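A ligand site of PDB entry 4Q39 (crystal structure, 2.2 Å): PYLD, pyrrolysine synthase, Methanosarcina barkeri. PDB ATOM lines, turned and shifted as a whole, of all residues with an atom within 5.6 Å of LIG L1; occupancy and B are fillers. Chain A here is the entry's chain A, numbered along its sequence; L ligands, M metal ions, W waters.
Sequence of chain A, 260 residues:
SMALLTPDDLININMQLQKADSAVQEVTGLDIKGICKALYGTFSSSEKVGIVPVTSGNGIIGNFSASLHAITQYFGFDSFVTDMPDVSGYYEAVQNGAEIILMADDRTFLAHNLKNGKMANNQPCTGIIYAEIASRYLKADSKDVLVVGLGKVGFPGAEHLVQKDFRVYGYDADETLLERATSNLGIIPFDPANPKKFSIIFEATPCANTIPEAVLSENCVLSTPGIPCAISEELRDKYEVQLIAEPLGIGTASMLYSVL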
ATOM      1  N   ALA A   3     -23.489  12.229  17.989  1.00  0.00           N
ATOM      2  CA  ALA A   3     -24.562  11.838  18.905  1.00  0.00           C
ATOM      3  C   ALA A   3     -23.978  11.773  20.303  1.00  0.00           C
ATOM      4  O   ALA A   3     -23.421  10.732  20.699  1.00  0.00           O
ATOM      5  CB  ALA A   3     -25.136  10.485  18.501  1.00  0.00           C
ATOM      6  N   LEU A   4     -24.047  12.880  21.030  1.00  0.00           N
ATOM      7  CA  LEU A   4     -23.417  12.963  22.343  1.00  0.00           C
ATOM      8  C   LEU A   4     -24.382  12.596  23.483  1.00  0.00           C
ATOM      9  O   LEU A   4     -25.555  12.937  23.455  1.00  0.00           O
ATOM     10  CB  LEU A   4     -22.878  14.358  22.587  1.00  0.00           C
ATOM     11  CG  LEU A   4     -21.822  14.867  21.593  1.00  0.00           C
ATOM     12  CD1 LEU A   4     -21.143  16.103  22.158  1.00  0.00           C
ATOM     13  CD2 LEU A   4     -20.790  13.812  21.222  1.00  0.00           C
ATOM     14  N   LEU A   5     -23.844  11.931  24.493  1.00  0.00           N
ATOM     15  CA  LEU A   5     -24.596  11.656  25.705  1.00  0.00           C
ATOM     16  C   LEU A   5     -25.239  12.912  26.247  1.00  0.00           C
ATOM     17  O   LEU A   5     -24.723  14.012  26.029  1.00  0.00           O
ATOM     18  CB  LEU A   5     -23.663  11.089  26.777  1.00  0.00           C
ATOM     19  CG  LEU A   5     -23.151   9.675  26.542  1.00  0.00           C
ATOM     20  CD1 LEU A   5     -22.106   9.352  27.575  1.00  0.00           C
ATOM     21  CD2 LEU A   5     -24.322   8.704  26.635  1.00  0.00           C
ATOM     22  N   ASN A 122     -12.556   5.049  22.938  1.00  0.00           N
ATOM     23  CA  ASN A 122     -13.879   4.506  23.284  1.00  0.00           C
ATOM     24  C   ASN A 122     -14.578   3.783  22.136  1.00  0.00           C
ATOM     25  O   ASN A 122     -15.260   2.773  22.340  1.00  0.00           O
ATOM     26  CB  ASN A 122     -14.766   5.629  23.770  1.00  0.00           C
ATOM     27  CG  ASN A 122     -16.162   5.178  24.090  1.00  0.00           C
ATOM     28  OD1 ASN A 122     -17.090   5.521  23.373  1.00  0.00           O
ATOM     29  ND2 ASN A 122     -16.317   4.444  25.185  1.00  0.00           N
ATOM     30  N   GLN A 123     -14.407   4.272  20.916  1.00  0.00           N
ATOM     31  CA  GLN A 123     -15.177   3.737  19.803  1.00  0.00           C
ATOM     32  C   GLN A 123     -14.911   2.277  19.476  1.00  0.00           C
ATOM     33  O   GLN A 123     -15.802   1.450  19.589  1.00  0.00           O
ATOM     34  CB  GLN A 123     -15.127   4.649  18.594  1.00  0.00           C
ATOM     35  CG  GLN A 123     -16.018   5.858  18.787  1.00  0.00           C
ATOM     36  CD  GLN A 123     -15.549   7.121  18.069  1.00  0.00           C
ATOM     37  OE1 GLN A 123     -14.416   7.204  17.573  1.00  0.00           O
ATOM     38  NE2 GLN A 123     -16.404   8.113  18.030  1.00  0.00           N
ATOM     39  N   THR A 126     -15.738  -0.086  22.587  1.00  0.00           N
ATOM     40  CA  THR A 126     -17.159  -0.321  22.710  1.00  0.00           C
ATOM     41  C   THR A 126     -17.622  -1.312  21.665  1.00  0.00           C
ATOM     42  O   THR A 126     -18.267  -2.301  21.995  1.00  0.00           O
ATOM     43  CB  THR A 126     -17.945   1.014  22.577  1.00  0.00           C
ATOM     44  OG1 THR A 126     -17.532   1.914  23.629  1.00  0.00           O
ATOM     45  CG2 THR A 126     -19.427   0.783  22.720  1.00  0.00           C
ATOM     46  N   TYR A 130     -19.116  -5.059  22.957  1.00  0.00           N
ATOM     47  CA  TYR A 130     -20.468  -5.422  22.667  1.00  0.00           C
ATOM     48  C   TYR A 130     -20.578  -6.572  21.654  1.00  0.00           C
ATOM     49  O   TYR A 130     -21.467  -7.441  21.771  1.00  0.00           O
ATOM     50  CB  TYR A 130     -21.286  -4.207  22.182  1.00  0.00           C
ATOM     51  CG  TYR A 130     -21.833  -3.371  23.314  1.00  0.00           C
ATOM     52  CD1 TYR A 130     -21.051  -2.396  23.923  1.00  0.00           C
ATOM     53  CD2 TYR A 130     -23.129  -3.553  23.789  1.00  0.00           C
ATOM     54  CE1 TYR A 130     -21.554  -1.611  24.945  1.00  0.00           C
ATOM     55  CE2 TYR A 130     -23.632  -2.779  24.819  1.00  0.00           C
ATOM     56  CZ  TYR A 130     -22.832  -1.813  25.390  1.00  0.00           C
ATOM     57  OH  TYR A 130     -23.329  -1.023  26.406  1.00  0.00           O
ATOM     58  N   VAL A 148     -26.270  -4.080  12.622  1.00  0.00           N
ATOM     59  CA  VAL A 148     -26.918  -2.859  12.079  1.00  0.00           C
ATOM     60  C   VAL A 148     -26.130  -1.635  12.585  1.00  0.00           C
ATOM     61  O   VAL A 148     -26.065  -1.385  13.788  1.00  0.00           O
ATOM     62  CB  VAL A 148     -28.390  -2.779  12.511  1.00  0.00           C
ATOM     63  CG1 VAL A 148     -29.062  -1.532  11.946  1.00  0.00           C
ATOM     64  CG2 VAL A 148     -29.148  -4.018  12.044  1.00  0.00           C
ATOM     65  N   GLY A 149     -25.493  -0.931  11.650  1.00  0.00           N
ATOM     66  CA  GLY A 149     -24.680   0.236  11.954  1.00  0.00           C
ATOM     67  C   GLY A 149     -23.222  -0.130  11.839  1.00  0.00           C
ATOM     68  O   GLY A 149     -22.741  -0.945  12.617  1.00  0.00           O
ATOM     69  N   LEU A 150     -22.534   0.472  10.880  1.00  0.00           N
ATOM     70  CA  LEU A 150     -21.143   0.123  10.584  1.00  0.00           C
ATOM     71  C   LEU A 150     -20.245   1.363  10.635  1.00  0.00           C
ATOM     72  O   LEU A 150     -19.335   1.502   9.848  1.00  0.00           O
ATOM     73  CB  LEU A 150     -21.058  -0.560   9.210  1.00  0.00           C
ATOM     74  CG  LEU A 150     -21.766  -1.934   9.183  1.00  0.00           C
ATOM     75  CD1 LEU A 150     -22.042  -2.409   7.771  1.00  0.00           C
ATOM     76  CD2 LEU A 150     -20.936  -2.962   9.929  1.00  0.00           C
ATOM     77  N   GLY A 151     -20.527   2.246  11.591  1.00  0.00           N
ATOM     78  CA  GLY A 151     -19.716   3.452  11.804  1.00  0.00           C
ATOM     79  C   GLY A 151     -18.531   3.244  12.713  1.00  0.00           C
ATOM     80  O   GLY A 151     -17.906   2.193  12.702  1.00  0.00           O
ATOM     81  N   LYS A 152     -18.227   4.253  13.508  1.00  0.00           N
ATOM     82  CA  LYS A 152     -17.038   4.225  14.376  1.00  0.00           C
ATOM     83  C   LYS A 152     -17.062   3.136  15.457  1.00  0.00           C
ATOM     84  O   LYS A 152     -16.011   2.613  15.831  1.00  0.00           O
ATOM     85  CB  LYS A 152     -16.816   5.632  14.954  1.00  0.00           C
ATOM     86  CG  LYS A 152     -16.310   6.622  13.876  1.00  0.00           C
ATOM     87  CD  LYS A 152     -16.020   8.012  14.414  1.00  0.00           C
ATOM     88  CE  LYS A 152     -17.137   9.009  14.085  1.00  0.00           C
ATOM     89  NZ  LYS A 152     -18.393   8.765  14.861  1.00  0.00           N
ATOM     90  N   VAL A 153     -18.266   2.806  15.952  1.00  0.00           N
ATOM     91  CA  VAL A 153     -18.491   1.698  16.878  1.00  0.00           C
ATOM     92  C   VAL A 153     -18.787   0.390  16.127  1.00  0.00           C
ATOM     93  O   VAL A 153     -18.168  -0.646  16.393  1.00  0.00           O
ATOM     94  CB  VAL A 153     -19.649   2.018  17.868  1.00  0.00           C
ATOM     95  CG1 VAL A 153     -20.000   0.833  18.729  1.00  0.00           C
ATOM     96  CG2 VAL A 153     -19.274   3.199  18.744  1.00  0.00           C
ATOM     97  N   GLY A 154     -19.703   0.450  15.183  1.00  0.00           N
ATOM     98  CA  GLY A 154     -20.163  -0.760  14.477  1.00  0.00           C
ATOM     99  C   GLY A 154     -19.093  -1.482  13.682  1.00  0.00           C
ATOM    100  O   GLY A 154     -18.993  -2.706  13.727  1.00  0.00           O
ATOM    101  N   TYR A 171     -25.822  -4.382   7.783  1.00  0.00           N
ATOM    102  CA  TYR A 171     -26.588  -3.344   7.134  1.00  0.00           C
ATOM    103  C   TYR A 171     -26.221  -1.988   7.731  1.00  0.00           C
ATOM    104  O   TYR A 171     -26.011  -1.865   8.945  1.00  0.00           O
ATOM    105  CB  TYR A 171     -28.077  -3.579   7.334  1.00  0.00           C
ATOM    106  CG  TYR A 171     -28.904  -2.509   6.659  1.00  0.00           C
ATOM    107  CD1 TYR A 171     -28.874  -2.347   5.277  1.00  0.00           C
ATOM    108  CD2 TYR A 171     -29.669  -1.626   7.414  1.00  0.00           C
ATOM    109  CE1 TYR A 171     -29.592  -1.351   4.665  1.00  0.00           C
ATOM    110  CE2 TYR A 171     -30.400  -0.627   6.806  1.00  0.00           C
ATOM    111  CZ  TYR A 171     -30.363  -0.502   5.421  1.00  0.00           C
ATOM    112  OH  TYR A 171     -31.071   0.493   4.819  1.00  0.00           O
ATOM    113  N   ASP A 172     -26.110  -0.977   6.855  1.00  0.00           N
ATOM    114  CA  ASP A 172     -26.009   0.427   7.262  1.00  0.00           C
ATOM    115  C   ASP A 172     -26.782   1.239   6.223  1.00  0.00           C
ATOM    116  O   ASP A 172     -26.708   0.943   5.038  1.00  0.00           O
ATOM    117  CB  ASP A 172     -24.553   0.895   7.293  1.00  0.00           C
ATOM    118  CG  ASP A 172     -24.393   2.238   7.954  1.00  0.00           C
ATOM    119  OD1 ASP A 172     -24.929   3.226   7.421  1.00  0.00           O
ATOM    120  OD2 ASP A 172     -23.732   2.305   9.035  1.00  0.00           O
ATOM    121  N   ALA A 173     -27.507   2.265   6.678  1.00  0.00           N
ATOM    122  CA  ALA A 173     -28.345   3.062   5.791  1.00  0.00           C
ATOM    123  C   ALA A 173     -27.523   3.907   4.851  1.00  0.00           C
ATOM    124  O   ALA A 173     -27.993   4.303   3.790  1.00  0.00           O
ATOM    125  CB  ALA A 173     -29.272   3.949   6.605  1.00  0.00           C
ATOM    126  N   ASP A 174     -26.295   4.210   5.245  1.00  0.00           N
ATOM    127  CA  ASP A 174     -25.358   4.845   4.335  1.00  0.00           C
ATOM    128  C   ASP A 174     -24.772   3.769   3.414  1.00  0.00           C
ATOM    129  O   ASP A 174     -23.981   2.932   3.843  1.00  0.00           O
ATOM    130  CB  ASP A 174     -24.266   5.555   5.133  1.00  0.00           C
ATOM    131  CG  ASP A 174     -23.263   6.280   4.250  1.00  0.00           C
ATOM    132  OD1 ASP A 174     -23.063   5.871   3.085  1.00  0.00           O
ATOM    133  OD2 ASP A 174     -22.652   7.243   4.727  1.00  0.00           O
ATOM    134  N   LEU A 177     -20.923   3.446   3.212  1.00  0.00           N
ATOM    135  CA  LEU A 177     -20.352   2.727   4.352  1.00  0.00           C
ATOM    136  C   LEU A 177     -20.562   1.235   4.180  1.00  0.00           C
ATOM    137  O   LEU A 177     -19.634   0.447   4.393  1.00  0.00           O
ATOM    138  CB  LEU A 177     -20.944   3.167   5.697  1.00  0.00           C
ATOM    139  CG  LEU A 177     -20.567   4.522   6.305  1.00  0.00           C
ATOM    140  CD1 LEU A 177     -20.568   4.406   7.823  1.00  0.00           C
ATOM    141  CD2 LEU A 177     -19.215   5.069   5.842  1.00  0.00           C
ATOM    142  N   ALA A 204     -25.386  -0.646  16.469  1.00  0.00           N
ATOM    143  CA  ALA A 204     -24.686   0.554  16.909  1.00  0.00           C
ATOM    144  C   ALA A 204     -25.051   1.763  16.047  1.00  0.00           C
ATOM    145  O   ALA A 204     -24.253   2.252  15.206  1.00  0.00           O
ATOM    146  CB  ALA A 204     -23.198   0.309  16.889  1.00  0.00           C
ATOM    147  N   THR A 205     -26.287   2.231  16.236  1.00  0.00           N
ATOM    148  CA  THR A 205     -26.736   3.471  15.591  1.00  0.00           C
ATOM    149  C   THR A 205     -27.278   4.467  16.618  1.00  0.00           C
ATOM    150  O   THR A 205     -27.618   4.095  17.741  1.00  0.00           O
ATOM    151  CB  THR A 205     -27.823   3.255  14.511  1.00  0.00           C
ATOM    152  OG1 THR A 205     -29.126   3.306  15.092  1.00  0.00           O
ATOM    153  CG2 THR A 205     -27.658   1.946  13.765  1.00  0.00           C
ATOM    154  N   PRO A 206     -27.396   5.731  16.227  1.00  0.00           N
ATOM    155  CA  PRO A 206     -28.008   6.723  17.103  1.00  0.00           C
ATOM    156  C   PRO A 206     -29.517   6.854  16.891  1.00  0.00           C
ATOM    157  O   PRO A 206     -30.094   7.889  17.231  1.00  0.00           O
ATOM    158  CB  PRO A 206     -27.276   8.005  16.696  1.00  0.00           C
ATOM    159  CG  PRO A 206     -27.028   7.821  15.235  1.00  0.00           C
ATOM    160  CD  PRO A 206     -26.752   6.364  15.057  1.00  0.00           C
ATOM    161  N   CYS A 207     -30.154   5.817  16.361  1.00  0.00           N
ATOM    162  CA  CYS A 207     -31.555   5.898  15.976  1.00  0.00           C
ATOM    163  C   CYS A 207     -32.422   4.855  16.676  1.00  0.00           C
ATOM    164  O   CYS A 207     -31.968   3.757  16.997  1.00  0.00           O
ATOM    165  CB  CYS A 207     -31.667   5.728  14.462  1.00  0.00           C
ATOM    166  SG  CYS A 207     -31.087   7.186  13.599  1.00  0.00           S
ATOM    167  N   THR A 210     -34.579   0.484  14.887  1.00  0.00           N
ATOM    168  CA  THR A 210     -33.821   0.099  13.685  1.00  0.00           C
ATOM    169  C   THR A 210     -33.832  -1.409  13.435  1.00  0.00           C
ATOM    170  O   THR A 210     -33.361  -1.868  12.396  1.00  0.00           O
ATOM    171  CB  THR A 210     -32.331   0.522  13.788  1.00  0.00           C
ATOM    172  OG1 THR A 210     -31.748  -0.022  14.977  1.00  0.00           O
ATOM    173  CG2 THR A 210     -32.212   2.024  13.781  1.00  0.00           C
ATOM    174  N   THR A 224     -26.435  -3.832  22.174  1.00  0.00           N
ATOM    175  CA  THR A 224     -26.470  -2.524  21.488  1.00  0.00           C
ATOM    176  C   THR A 224     -26.000  -1.364  22.368  1.00  0.00           C
ATOM    177  O   THR A 224     -26.632  -1.055  23.397  1.00  0.00           O
ATOM    178  CB  THR A 224     -27.886  -2.212  20.929  1.00  0.00           C
ATOM    179  OG1 THR A 224     -27.886  -0.950  20.262  1.00  0.00           O
ATOM    180  CG2 THR A 224     -28.961  -2.206  22.036  1.00  0.00           C
ATOM    181  N   PRO A 225     -24.880  -0.732  21.984  1.00  0.00           N
ATOM    182  CA  PRO A 225     -24.466   0.485  22.678  1.00  0.00           C
ATOM    183  C   PRO A 225     -25.208   1.722  22.160  1.00  0.00           C
ATOM    184  O   PRO A 225     -25.148   2.793  22.784  1.00  0.00           O
ATOM    185  CB  PRO A 225     -22.972   0.586  22.327  1.00  0.00           C
ATOM    186  CG  PRO A 225     -22.838  -0.119  21.040  1.00  0.00           C
ATOM    187  CD  PRO A 225     -23.843  -1.224  21.062  1.00  0.00           C
ATOM    188  N   GLY A 226     -25.922   1.552  21.058  1.00  0.00           N
ATOM    189  CA  GLY A 226     -26.654   2.655  20.414  1.00  0.00           C
ATOM    190  C   GLY A 226     -27.660   3.317  21.318  1.00  0.00           C
ATOM    191  O   GLY A 226     -28.229   2.694  22.207  1.00  0.00           O
ATOM    192  N   ILE A 227     -27.889   4.598  21.088  1.00  0.00           N
ATOM    193  CA  ILE A 227     -28.828   5.392  21.883  1.00  0.00           C
ATOM    194  C   ILE A 227     -29.607   6.319  20.945  1.00  0.00           C
ATOM    195  O   ILE A 227     -28.988   7.000  20.123  1.00  0.00           O
ATOM    196  CB  ILE A 227     -28.081   6.274  22.923  1.00  0.00           C
ATOM    197  CG1 ILE A 227     -27.369   5.413  23.956  1.00  0.00           C
ATOM    198  CG2 ILE A 227     -29.037   7.193  23.661  1.00  0.00           C
ATOM    199  CD1 ILE A 227     -26.326   6.189  24.751  1.00  0.00           C
ATOM    200  N   PRO A 228     -30.943   6.374  21.070  1.00  0.00           N
ATOM    201  CA  PRO A 228     -31.819   5.631  21.996  1.00  0.00           C
ATOM    202  C   PRO A 228     -31.935   4.159  21.605  1.00  0.00           C
ATOM    203  O   PRO A 228     -31.173   3.677  20.755  1.00  0.00           O
ATOM    204  CB  PRO A 228     -33.169   6.360  21.873  1.00  0.00           C
ATOM    205  CG  PRO A 228     -33.139   6.991  20.539  1.00  0.00           C
ATOM    206  CD  PRO A 228     -31.703   7.348  20.258  1.00  0.00           C
ATOM    207  N   GLU A 246     -26.457  -0.160  27.619  1.00  0.00           N
ATOM    208  CA  GLU A 246     -26.000   0.595  28.759  1.00  0.00           C
ATOM    209  C   GLU A 246     -25.197   1.763  28.188  1.00  0.00           C
ATOM    210  O   GLU A 246     -24.532   1.602  27.195  1.00  0.00           O
ATOM    211  CB  GLU A 246     -25.169  -0.348  29.625  1.00  0.00           C
ATOM    212  CG  GLU A 246     -24.651   0.249  30.894  1.00  0.00           C
ATOM    213  CD  GLU A 246     -23.376   1.031  30.665  1.00  0.00           C
ATOM    214  OE1 GLU A 246     -22.620   0.728  29.714  1.00  0.00           O
ATOM    215  OE2 GLU A 246     -23.133   1.961  31.450  1.00  0.00           O
ATOM    216  N   PRO A 247     -25.288   2.951  28.786  1.00  0.00           N
ATOM    217  CA  PRO A 247     -24.840   4.158  28.051  1.00  0.00           C
ATOM    218  C   PRO A 247     -23.357   4.529  28.104  1.00  0.00           C
ATOM    219  O   PRO A 247     -22.911   5.349  27.301  1.00  0.00           O
ATOM    220  CB  PRO A 247     -25.676   5.277  28.676  1.00  0.00           C
ATOM    221  CG  PRO A 247     -25.902   4.778  30.080  1.00  0.00           C
ATOM    222  CD  PRO A 247     -26.150   3.310  29.918  1.00  0.00           C
ATOM    223  N   LEU A 248     -22.584   3.936  29.011  1.00  0.00           N
ATOM    224  CA  LEU A 248     -21.186   4.364  29.184  1.00  0.00           C
ATOM    225  C   LEU A 248     -20.228   3.313  29.782  1.00  0.00           C
ATOM    226  O   LEU A 248     -19.079   3.214  29.346  1.00  0.00           O
ATOM    227  CB  LEU A 248     -21.161   5.658  30.010  1.00  0.00           C
ATOM    228  CG  LEU A 248     -19.821   6.371  30.207  1.00  0.00           C
ATOM    229  CD1 LEU A 248     -19.225   6.796  28.869  1.00  0.00           C
ATOM    230  CD2 LEU A 248     -19.997   7.586  31.102  1.00  0.00           C
ATOM    231  N   GLY A 249     -20.697   2.542  30.752  1.00  0.00           N
ATOM    232  CA  GLY A 249     -19.857   1.655  31.587  1.00  0.00           C
ATOM    233  C   GLY A 249     -19.146   0.480  30.948  1.00  0.00           C
ATOM    234  O   GLY A 249     -17.993   0.201  31.222  1.00  0.00           O
ATOM    235  N   GLY A 251     -18.413   0.042  27.712  1.00  0.00           N
ATOM    236  CA  GLY A 251     -17.359   0.560  26.841  1.00  0.00           C
ATOM    237  C   GLY A 251     -16.191   1.123  27.626  1.00  0.00           C
ATOM    238  O   GLY A 251     -15.018   0.940  27.217  1.00  0.00           O
HETATM  239  P1  LIG L   1     -21.502   6.691  13.731  1.00  0.00           P
HETATM  240  O1  LIG L   1     -22.338   7.838  13.275  1.00  0.00           O
HETATM  241  O2  LIG L   1     -20.063   6.555  13.404  1.00  0.00           O
HETATM  242  O3  LIG L   1     -22.187   5.351  13.179  1.00  0.00           O
HETATM  243  C1  LIG L   1     -23.597   5.205  13.233  1.00  0.00           C
HETATM  244  C2  LIG L   1     -23.992   4.466  11.954  1.00  0.00           C
HETATM  245  O4  LIG L   1     -25.342   4.055  12.035  1.00  0.00           O
HETATM  246  C3  LIG L   1     -23.881   5.374  10.726  1.00  0.00           C
HETATM  247  O5  LIG L   1     -23.026   4.752   9.786  1.00  0.00           O
HETATM  248  C4  LIG L   1     -25.274   5.507  10.170  1.00  0.00           C
HETATM  249  O6  LIG L   1     -25.275   5.421   8.746  1.00  0.00           O
HETATM  250  C5  LIG L   1     -25.907   4.259  10.734  1.00  0.00           C
HETATM  251  N1  LIG L   1     -27.372   4.316  10.817  1.00  0.00           N
HETATM  252  C6  LIG L   1     -28.172   5.280  11.308  1.00  0.00           C
HETATM  253  N2  LIG L   1     -29.480   4.898  11.221  1.00  0.00           N
HETATM  254  C7  LIG L   1     -29.500   3.687  10.669  1.00  0.00           C
HETATM  255  C8  LIG L   1     -30.516   2.707  10.269  1.00  0.00           C
HETATM  256  N3  LIG L   1     -31.816   2.934  10.451  1.00  0.00           N
HETATM  257  N4  LIG L   1     -30.098   1.552   9.742  1.00  0.00           N
HETATM  258  C9  LIG L   1     -28.809   1.268   9.554  1.00  0.00           C
HETATM  259  N5  LIG L   1     -27.840   2.113   9.863  1.00  0.00           N
HETATM  260  C10 LIG L   1     -28.126   3.307  10.415  1.00  0.00           C
HETATM  261  O7  LIG L   1     -21.845   6.619  15.324  1.00  0.00           O
HETATM  262  P2  LIG L   1     -20.937   5.773  16.335  1.00  0.00           P
HETATM  263  O8  LIG L   1     -19.731   6.516  16.846  1.00  0.00           O
HETATM  264  O9  LIG L   1     -20.672   4.394  15.730  1.00  0.00           O
HETATM  265  O10 LIG L   1     -21.980   5.678  17.567  1.00  0.00           O
HETATM  266  C11 LIG L   1     -23.138   4.885  17.410  1.00  0.00           C
HETATM  267  C12 LIG L   1     -24.011   5.062  18.639  1.00  0.00           C
HETATM  268  O11 LIG L   1     -23.413   4.551  19.838  1.00  0.00           O
HETATM  269  C13 LIG L   1     -24.323   6.499  18.949  1.00  0.00           C
HETATM  270  O12 LIG L   1     -25.663   6.489  19.458  1.00  0.00           O
HETATM  271  C14 LIG L   1     -23.404   6.871  20.084  1.00  0.00           C
HETATM  272  O13 LIG L   1     -24.001   7.859  20.905  1.00  0.00           O
HETATM  273  C15 LIG L   1     -23.381   5.579  20.854  1.00  0.00           C
HETATM  274  N6  LIG L   1     -22.249   5.238  21.699  1.00  0.00           N
HETATM  275  C16 LIG L   1     -22.551   4.567  22.816  1.00  0.00           C
HETATM  276  C17 LIG L   1     -21.575   4.105  23.679  1.00  0.00           C
HETATM  277  C18 LIG L   1     -21.961   3.328  24.906  1.00  0.00           C
HETATM  278  O14 LIG L   1     -21.075   3.054  25.733  1.00  0.00           O
HETATM  279  N7  LIG L   1     -23.209   2.891  25.082  1.00  0.00           N
HETATM  280  C19 LIG L   1     -20.120   4.342  23.375  1.00  0.00           C
HETATM  281  C20 LIG L   1     -19.915   5.058  22.119  1.00  0.00           C
HETATM  282  C21 LIG L   1     -20.977   5.472  21.324  1.00  0.00           C
HETATM  283  C1  LG2 L   2     -18.313   8.707  25.328  1.00  0.00           C
HETATM  284  C2  LG2 L   2     -19.744   8.962  24.945  1.00  0.00           C
HETATM  285  C3  LG2 L   2     -20.516   7.694  24.607  1.00  0.00           C
HETATM  286  C4  LG2 L   2     -21.332   8.123  23.422  1.00  0.00           C
HETATM  287  N1  LG2 L   2     -20.987   9.267  22.980  1.00  0.00           N
HETATM  288  C5  LG2 L   2     -19.813   9.791  23.674  1.00  0.00           C
HETATM  289  C6  LG2 L   2     -19.912  11.204  24.100  1.00  0.00           C
HETATM  290  O1  LG2 L   2     -21.011  11.603  24.454  1.00  0.00           O
HETATM  291  N2  LG2 L   2     -18.774  11.908  24.096  1.00  0.00           N
HETATM  292  C7  LG2 L   2     -18.733  13.305  24.531  1.00  0.00           C
HETATM  293  C8  LG2 L   2     -18.327  13.416  25.988  1.00  0.00           C
HETATM  294  C9  LG2 L   2     -17.853  14.802  26.355  1.00  0.00           C
HETATM  295  C10 LG2 L   2     -17.453  14.878  27.813  1.00  0.00           C
HETATM  296  C11 LG2 L   2     -17.254  16.311  28.317  1.00  0.00           C
HETATM  297  C12 LG2 L   2     -16.956  16.275  29.792  1.00  0.00           C
HETATM  298  O2  LG2 L   2     -17.934  16.246  30.590  1.00  0.00           O
HETATM  299  O3  LG2 L   2     -15.751  16.237  30.195  1.00  0.00           O
HETATM  300  N3  LG2 L   2     -16.174  16.945  27.585  1.00  0.00           N
HETATM  301 MG    MG M   1     -21.371   0.958  27.361  1.00  0.00          MG
HETATM  302  O   HOH W   1     -18.687   3.714  26.586  1.00  0.00           O
HETATM  303  O   HOH W   2     -26.982   9.110  20.709  1.00  0.00           O
HETATM  304  O   HOH W   3     -19.107   7.163  10.969  1.00  0.00           O
HETATM  305  O   HOH W   4     -19.043   7.553  19.179  1.00  0.00           O
HETATM  306  O   HOH W   5     -24.717   8.838  12.046  1.00  0.00           O
HETATM  307  O   HOH W   6     -27.341   8.422  12.104  1.00  0.00           O
HETATM  308  O   HOH W   7     -17.628   7.634  21.690  1.00  0.00           O
HETATM  309  O   HOH W   8     -21.777   2.504  14.277  1.00  0.00           O
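A nitrogen (N7) of LIG L1 is in hydrogen-bond range of the backbone carbonyl oxygen of Glu 246 (2.8 Å).
O2 of LIG L1 is in salt-bridge range of NZ of Lys 152, 3.1 Å away.
The side-chain carboxylate (OD1) of Asp 172 is in hydrogen-bond range of an oxygen (O6) of LIG L1.
O12 of LIG L1 is in hydrogen-bond range of O of Ile 227 (3.4 Å).
An oxygen (O12) of LIG L1 sits at hydrogen-bond distance from the backbone NH (N) of Ile 227, 3.3 Å away.
The backbone carbonyl oxygen (O) of Pro 225 is in hydrogen-bond range of a nitrogen (N7) of LIG L1 (3.0 Å).
A nitrogen (N2) of LIG L1 is in hydrogen-bond range of the side-chain sulfur (SG) of Cys 207 (3.7 Å).
N of Lys 152 sits at hydrogen-bond distance from O2 of LIG L1.
N5 of LIG L1 lies within hydrogen-bond range of N of Ala 173 (3.2 Å).
The backbone NH (N) of Leu 5 sits at hydrogen-bond distance from an oxygen (O1) of LG2 L2 (2.9 Å).
The backbone carbonyl oxygen (O) of Ala 3 is in hydrogen-bond range of an oxygen (O13) of LIG L1 (2.9 Å).
N of Val 153 is in hydrogen-bond range of O9 of LIG L1 (2.9 Å).
O of Pro 247 sits close to N7 of LIG L1, at 3.3 Å.
OD1 of Asp 172 sits at hydrogen-bond distance from N of Asp 174 (2.8 Å).
N of Cys 207 is in hydrogen-bond range of OG1 of Thr 205 (3.0 Å).
OE2 of Glu 246 is in hydrogen-bond range of N of Gly 249, 2.6 Å away.
N of Ile 227 lies within hydrogen-bond range of O of Thr 205, 3.4 Å away.
The side-chain carboxylate (OD2) of Asp 172 lies within hydrogen-bond range of the backbone NH (N) of Leu 150, at 2.9 Å.
N of Leu 177 is in hydrogen-bond range of OD1 of Asp 174 (3.2 Å).
O of Val 148 lies within hydrogen-bond range of N of Ala 204 (2.9 Å).
O of Asn 122 is in hydrogen-bond range of OG1 of Thr 126 (2.7 Å).
Residues that only touch LIG L1: Asn 122, Gln 123, Thr 126, Val 148, Gly 149, Gly 151, Tyr 171, Asp 174, Leu 177, Ala 204, Thr 205, Pro 206, Thr 210, Gly 226 and Leu 248.
Hydrophobic or aromatic side chains within 4 Å of LIG L1: Ala 3, Val 148, Val 153, Tyr 171, Leu 177, Pro 206 and Pro 225.
Along chain A the residues within 4 Å of LIG L1 span positions 3 to 248.
Water W1 lies within hydrogen-bond range of an oxygen (O14) of LIG L1, the backbone carbonyl oxygen of Leu 248 and the side-chain amide nitrogen of Asn 122.
Water W8 lies within hydrogen-bond range of an oxygen (O9) of LIG L1 (2.6 Å), the backbone carbonyl oxygen (O) of Ala 204 (2.7 Å), the backbone NH (N) of Gly 151 (3.0 Å) and the backbone NH (N) of Gly 154 (3.1 Å).
Water W4 lies within hydrogen-bond range of an oxygen (O8) of LIG L1 (2.6 Å) and the side-chain amide nitrogen (NE2) of Gln 123 (2.9 Å).
Water W2 bridges the backbone carbonyl oxygen of Ile 227 (3.0 Å) and an oxygen (O12) of LIG L1 (3.2 Å).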
